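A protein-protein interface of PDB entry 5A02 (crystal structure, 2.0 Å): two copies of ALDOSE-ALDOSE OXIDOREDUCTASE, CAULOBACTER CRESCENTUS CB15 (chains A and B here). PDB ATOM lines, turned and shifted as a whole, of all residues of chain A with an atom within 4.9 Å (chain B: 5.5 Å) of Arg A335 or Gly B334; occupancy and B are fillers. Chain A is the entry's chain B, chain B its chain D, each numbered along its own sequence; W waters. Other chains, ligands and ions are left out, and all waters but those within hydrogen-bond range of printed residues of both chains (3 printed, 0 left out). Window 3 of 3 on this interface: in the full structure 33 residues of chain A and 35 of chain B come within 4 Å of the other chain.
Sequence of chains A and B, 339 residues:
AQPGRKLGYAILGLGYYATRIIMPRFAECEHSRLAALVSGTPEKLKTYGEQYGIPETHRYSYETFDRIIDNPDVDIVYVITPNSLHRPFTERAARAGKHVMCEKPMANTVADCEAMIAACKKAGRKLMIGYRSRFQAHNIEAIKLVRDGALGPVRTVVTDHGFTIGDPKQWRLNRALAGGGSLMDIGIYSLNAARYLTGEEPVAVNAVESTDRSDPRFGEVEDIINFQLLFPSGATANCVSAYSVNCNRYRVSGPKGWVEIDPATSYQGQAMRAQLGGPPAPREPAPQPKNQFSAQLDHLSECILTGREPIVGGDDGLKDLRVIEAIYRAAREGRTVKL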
ATOM      1  N   VAL A 205      -1.883   6.216 -29.199  1.00  0.00           N
ATOM      2  CA  VAL A 205      -1.992   4.821 -28.755  1.00  0.00           C
ATOM      3  C   VAL A 205      -1.728   4.668 -27.251  1.00  0.00           C
ATOM      4  O   VAL A 205      -0.706   5.133 -26.747  1.00  0.00           O
ATOM      5  CB  VAL A 205      -0.988   3.918 -29.535  1.00  0.00           C
ATOM      6  CG1 VAL A 205      -1.073   2.481 -29.072  1.00  0.00           C
ATOM      7  CG2 VAL A 205      -1.235   4.010 -31.041  1.00  0.00           C
ATOM      8  N   ASN A 206      -2.659   4.026 -26.542  1.00  0.00           N
ATOM      9  CA  ASN A 206      -2.420   3.483 -25.204  1.00  0.00           C
ATOM     10  C   ASN A 206      -2.382   1.954 -25.232  1.00  0.00           C
ATOM     11  O   ASN A 206      -3.020   1.332 -26.084  1.00  0.00           O
ATOM     12  CB  ASN A 206      -3.517   3.905 -24.229  1.00  0.00           C
ATOM     13  CG  ASN A 206      -3.316   5.293 -23.675  1.00  0.00           C
ATOM     14  OD1 ASN A 206      -2.209   5.839 -23.691  1.00  0.00           O
ATOM     15  ND2 ASN A 206      -4.394   5.872 -23.165  1.00  0.00           N
ATOM     16  N   ARG A 329       5.352  -0.217 -27.425  1.00  0.00           N
ATOM     17  CA  ARG A 329       6.036   0.884 -26.751  1.00  0.00           C
ATOM     18  C   ARG A 329       5.159   1.491 -25.658  1.00  0.00           C
ATOM     19  O   ARG A 329       5.615   1.688 -24.544  1.00  0.00           O
ATOM     20  CB  ARG A 329       6.457   1.964 -27.754  1.00  0.00           C
ATOM     21  CG  ARG A 329       7.291   3.094 -27.118  1.00  0.00           C
ATOM     22  CD  ARG A 329       7.774   4.107 -28.159  1.00  0.00           C
ATOM     23  NE  ARG A 329       8.485   3.432 -29.237  1.00  0.00           N
ATOM     24  CZ  ARG A 329       8.062   3.357 -30.498  1.00  0.00           C
ATOM     25  NH1 ARG A 329       6.925   3.943 -30.872  1.00  0.00           N
ATOM     26  NH2 ARG A 329       8.789   2.697 -31.391  1.00  0.00           N
ATOM     27  N   ALA A 330       3.894   1.763 -25.968  1.00  0.00           N
ATOM     28  CA  ALA A 330       2.973   2.309 -24.971  1.00  0.00           C
ATOM     29  C   ALA A 330       2.823   1.427 -23.732  1.00  0.00           C
ATOM     30  O   ALA A 330       2.737   1.925 -22.603  1.00  0.00           O
ATOM     31  CB  ALA A 330       1.594   2.554 -25.609  1.00  0.00           C
ATOM     32  N   GLU A 333       6.298   1.581 -21.834  1.00  0.00           N
ATOM     33  CA  GLU A 333       6.646   2.848 -21.195  1.00  0.00           C
ATOM     34  C   GLU A 333       5.532   3.423 -20.347  1.00  0.00           C
ATOM     35  O   GLU A 333       5.743   4.386 -19.613  1.00  0.00           O
ATOM     36  CB  GLU A 333       7.059   3.867 -22.251  1.00  0.00           C
ATOM     37  CG  GLU A 333       8.217   3.403 -23.122  1.00  0.00           C
ATOM     38  CD  GLU A 333       8.703   4.490 -24.060  1.00  0.00           C
ATOM     39  OE1 GLU A 333       8.095   5.576 -24.074  1.00  0.00           O
ATOM     40  OE2 GLU A 333       9.687   4.263 -24.790  1.00  0.00           O
ATOM     41  N   GLY A 334       4.339   2.848 -20.446  1.00  0.00           N
ATOM     42  CA  GLY A 334       3.218   3.349 -19.674  1.00  0.00           C
ATOM     43  C   GLY A 334       2.850   4.778 -20.018  1.00  0.00           C
ATOM     44  O   GLY A 334       2.601   5.598 -19.133  1.00  0.00           O
ATOM     45  N   ARG A 335       2.804   5.081 -21.310  1.00  0.00           N
ATOM     46  CA  ARG A 335       2.383   6.404 -21.760  1.00  0.00           C
ATOM     47  C   ARG A 335       1.667   6.323 -23.100  1.00  0.00           C
ATOM     48  O   ARG A 335       1.777   5.331 -23.819  1.00  0.00           O
ATOM     49  CB  ARG A 335       3.585   7.347 -21.871  1.00  0.00           C
ATOM     50  CG  ARG A 335       4.685   6.805 -22.744  1.00  0.00           C
ATOM     51  CD  ARG A 335       5.798   7.818 -22.994  1.00  0.00           C
ATOM     52  NE  ARG A 335       6.673   7.387 -24.089  1.00  0.00           N
ATOM     53  CZ  ARG A 335       6.545   7.779 -25.358  1.00  0.00           C
ATOM     54  NH1 ARG A 335       5.583   8.635 -25.710  1.00  0.00           N
ATOM     55  NH2 ARG A 335       7.392   7.325 -26.277  1.00  0.00           N
ATOM     56  N   THR A 336       0.929   7.376 -23.426  1.00  0.00           N
ATOM     57  CA  THR A 336       0.309   7.508 -24.735  1.00  0.00           C
ATOM     58  C   THR A 336       1.382   7.784 -25.785  1.00  0.00           C
ATOM     59  O   THR A 336       2.124   8.757 -25.682  1.00  0.00           O
ATOM     60  CB  THR A 336      -0.738   8.641 -24.732  1.00  0.00           C
ATOM     61  OG1 THR A 336      -1.657   8.441 -23.651  1.00  0.00           O
ATOM     62  CG2 THR A 336      -1.496   8.695 -26.055  1.00  0.00           C
ATOM     63  N   VAL A 337       1.479   6.914 -26.784  1.00  0.00           N
ATOM     64  CA  VAL A 337       2.438   7.095 -27.864  1.00  0.00           C
ATOM     65  C   VAL A 337       1.781   7.813 -29.050  1.00  0.00           C
ATOM     66  O   VAL A 337       0.718   7.409 -29.527  1.00  0.00           O
ATOM     67  CB  VAL A 337       3.021   5.738 -28.327  1.00  0.00           C
ATOM     68  CG1 VAL A 337       3.909   5.922 -29.549  1.00  0.00           C
ATOM     69  CG2 VAL A 337       3.791   5.073 -27.191  1.00  0.00           C
ATOM     70  N   ASN B 206      -5.261   3.547 -17.891  1.00  0.00           N
ATOM     71  CA  ASN B 206      -5.077   4.369 -19.103  1.00  0.00           C
ATOM     72  C   ASN B 206      -6.401   5.008 -19.494  1.00  0.00           C
ATOM     73  O   ASN B 206      -7.464   4.465 -19.179  1.00  0.00           O
ATOM     74  CB  ASN B 206      -4.580   3.548 -20.298  1.00  0.00           C
ATOM     75  CG  ASN B 206      -3.085   3.330 -20.303  1.00  0.00           C
ATOM     76  OD1 ASN B 206      -2.311   4.131 -19.771  1.00  0.00           O
ATOM     77  ND2 ASN B 206      -2.664   2.241 -20.935  1.00  0.00           N
ATOM     78  N   ARG B 329      -7.149  11.947 -14.979  1.00  0.00           N
ATOM     79  CA  ARG B 329      -5.741  12.323 -14.972  1.00  0.00           C
ATOM     80  C   ARG B 329      -4.977  11.626 -16.095  1.00  0.00           C
ATOM     81  O   ARG B 329      -4.162  12.243 -16.768  1.00  0.00           O
ATOM     82  CB  ARG B 329      -5.118  11.995 -13.613  1.00  0.00           C
ATOM     83  CG  ARG B 329      -3.649  12.409 -13.451  1.00  0.00           C
ATOM     84  CD  ARG B 329      -3.174  12.149 -12.013  1.00  0.00           C
ATOM     85  NE  ARG B 329      -3.982  12.910 -11.053  1.00  0.00           N
ATOM     86  CZ  ARG B 329      -4.784  12.376 -10.127  1.00  0.00           C
ATOM     87  NH1 ARG B 329      -4.886  11.051  -9.986  1.00  0.00           N
ATOM     88  NH2 ARG B 329      -5.483  13.177  -9.323  1.00  0.00           N
ATOM     89  N   ALA B 330      -5.266  10.341 -16.302  1.00  0.00           N
ATOM     90  CA  ALA B 330      -4.614   9.562 -17.352  1.00  0.00           C
ATOM     91  C   ALA B 330      -4.895  10.147 -18.727  1.00  0.00           C
ATOM     92  O   ALA B 330      -4.004  10.223 -19.574  1.00  0.00           O
ATOM     93  CB  ALA B 330      -5.072   8.085 -17.284  1.00  0.00           C
ATOM     94  N   ALA B 331      -6.136  10.572 -18.945  1.00  0.00           N
ATOM     95  CA  ALA B 331      -6.510  11.168 -20.218  1.00  0.00           C
ATOM     96  C   ALA B 331      -5.852  12.530 -20.408  1.00  0.00           C
ATOM     97  O   ALA B 331      -5.455  12.888 -21.516  1.00  0.00           O
ATOM     98  CB  ALA B 331      -8.041  11.302 -20.322  1.00  0.00           C
ATOM     99  N   ARG B 332      -5.755  13.299 -19.333  1.00  0.00           N
ATOM    100  CA  ARG B 332      -5.178  14.633 -19.429  1.00  0.00           C
ATOM    101  C   ARG B 332      -3.665  14.572 -19.658  1.00  0.00           C
ATOM    102  O   ARG B 332      -3.120  15.320 -20.471  1.00  0.00           O
ATOM    103  CB  ARG B 332      -5.497  15.441 -18.164  1.00  0.00           C
ATOM    104  CG  ARG B 332      -4.938  16.862 -18.170  1.00  0.00           C
ATOM    105  CD  ARG B 332      -5.438  17.643 -16.961  1.00  0.00           C
ATOM    106  NE  ARG B 332      -5.009  17.030 -15.709  1.00  0.00           N
ATOM    107  CZ  ARG B 332      -5.823  16.459 -14.823  1.00  0.00           C
ATOM    108  NH1 ARG B 332      -7.139  16.415 -15.033  1.00  0.00           N
ATOM    109  NH2 ARG B 332      -5.312  15.936 -13.713  1.00  0.00           N
ATOM    110  N   GLU B 333      -2.993  13.662 -18.963  1.00  0.00           N
ATOM    111  CA  GLU B 333      -1.531  13.614 -18.980  1.00  0.00           C
ATOM    112  C   GLU B 333      -0.954  12.675 -20.038  1.00  0.00           C
ATOM    113  O   GLU B 333       0.252  12.705 -20.328  1.00  0.00           O
ATOM    114  CB  GLU B 333      -1.016  13.212 -17.593  1.00  0.00           C
ATOM    115  CG  GLU B 333      -1.315  14.263 -16.535  1.00  0.00           C
ATOM    116  CD  GLU B 333      -0.694  13.959 -15.177  1.00  0.00           C
ATOM    117  OE1 GLU B 333      -0.016  12.918 -15.034  1.00  0.00           O
ATOM    118  OE2 GLU B 333      -0.907  14.765 -14.243  1.00  0.00           O
ATOM    119  N   GLY B 334      -1.805  11.830 -20.611  1.00  0.00           N
ATOM    120  CA  GLY B 334      -1.335  10.863 -21.589  1.00  0.00           C
ATOM    121  C   GLY B 334      -0.343   9.870 -21.010  1.00  0.00           C
ATOM    122  O   GLY B 334       0.709   9.602 -21.596  1.00  0.00           O
ATOM    123  N   ARG B 335      -0.677   9.310 -19.856  1.00  0.00           N
ATOM    124  CA  ARG B 335       0.182   8.310 -19.241  1.00  0.00           C
ATOM    125  C   ARG B 335      -0.616   7.329 -18.397  1.00  0.00           C
ATOM    126  O   ARG B 335      -1.767   7.584 -18.036  1.00  0.00           O
ATOM    127  CB  ARG B 335       1.254   8.984 -18.382  1.00  0.00           C
ATOM    128  CG  ARG B 335       0.689   9.627 -17.147  1.00  0.00           C
ATOM    129  CD  ARG B 335       1.783  10.210 -16.258  1.00  0.00           C
ATOM    130  NE  ARG B 335       1.205  10.855 -15.082  1.00  0.00           N
ATOM    131  CZ  ARG B 335       0.958  10.229 -13.935  1.00  0.00           C
ATOM    132  NH1 ARG B 335       1.247   8.937 -13.803  1.00  0.00           N
ATOM    133  NH2 ARG B 335       0.427  10.897 -12.919  1.00  0.00           N
ATOM    134  N   THR B 336      -0.009   6.190 -18.096  1.00  0.00           N
ATOM    135  CA  THR B 336      -0.631   5.221 -17.203  1.00  0.00           C
ATOM    136  C   THR B 336      -0.552   5.721 -15.765  1.00  0.00           C
ATOM    137  O   THR B 336       0.536   5.965 -15.247  1.00  0.00           O
ATOM    138  CB  THR B 336       0.051   3.850 -17.307  1.00  0.00           C
ATOM    139  OG1 THR B 336       0.076   3.445 -18.680  1.00  0.00           O
ATOM    140  CG2 THR B 336      -0.696   2.805 -16.466  1.00  0.00           C
HETATM  141  O   HOH W   1      -0.837   5.944 -21.203  1.00  0.00           O
HETATM  142  O   HOH W   2      -0.117   3.014 -22.450  1.00  0.00           O
HETATM  143  O   HOH W   3      -3.694   7.485 -20.621  1.00  0.00           O
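O of Gly A334 sits at hydrogen-bond distance from N of Thr B336 (2.9 Å). N of Thr A336 lies within hydrogen-bond range of O of Gly B334, 2.9 Å away.
OG1 of Thr A336 is in hydrogen-bond range of OD1 of Asn A206 (2.7 Å). The side-chain carboxylate (OE1) of Glu B333 lies within salt-bridge range of the guanidinium group (NH2) of Arg B335. OE1 of Glu A333 is in salt-bridge range of NH2 of Arg A335 (2.9 Å). OG1 of Thr B336 lies within hydrogen-bond range of OD1 of Asn B206, 2.7 Å away. N of Arg A335 is in hydrogen-bond range of O of Ala A330 (3.4 Å). The backbone NH (N) of Arg B335 sits at hydrogen-bond distance from the backbone carbonyl oxygen (O) of Ala B330.
Asn B206 touches Asn A206. Gly A334 touches Arg B335. Arg A335 touches Gly B334 (CA to O, 3.6 Å). CA of Arg B335 touches CA of Arg A335, at 3.9 Å.
Of chain A, only Arg A335 and Thr A336 come within 4 Å of Gly B334. Of the printed residues of chain B, Thr A336 touches Gly B334 (2.9 Å). Printed residues of chain A within 4 Å of Thr B336: Gly A334 (2.9 Å). Of the printed residues of chain B, Gly A334 touches Arg B335 and Thr B336. Printed residues of chain A within 4 Å of Arg B335: Gly A334 (3.6 Å) and Arg A335 (3.9 Å). Printed residues of chain A within 4 Å of Asn B206: Asn A206. Arg B332 touches none of the printed residues of chain A.
Of the 9 printed residues of chain B, 4 touch a printed residue of chain A. Printed residues of chain B that touch a printed residue of chain A: Asn B206, Gly B334, Arg B335 and Thr B336. Printed residues of chain A that touch a printed residue of chain B: Asn A206, Gly A334, Arg A335 and Thr A336. Among the printed residues, 6 pairs touch across the chains.
Asn B206 touches its own counterpart, Asn A206. Gly A334 touches Arg B335, and with the chains exchanged Arg A335 touches Gly B334. Gly A334 touches Thr B336, and with the chains exchanged Thr A336 touches Gly B334. Arg B335 touches its own counterpart, Arg A335. Of the 6 pairs that touch across the chains among the printed residues, 6 have their exchanged pair printed and touching as well.
Water W1 lies within hydrogen-bond range of the side-chain amide oxygen (OD1) of Asn B206 (2.7 Å), the side-chain amide oxygen (OD1) of Asn A206 (2.8 Å), the backbone NH (N) of Thr A336 (3.2 Å) and the backbone NH (N) of Thr B336 (3.2 Å). Water W3 lies within hydrogen-bond range of the backbone carbonyl oxygen of Ala B330, the side-chain amide nitrogen of Asn A206 and the backbone carbonyl oxygen of Arg B335. Water W2 lies within hydrogen-bond range of O of Ala A330 (3.1 Å), ND2 of Asn B206 (3.1 Å) and O of Arg A335 (3.3 Å).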
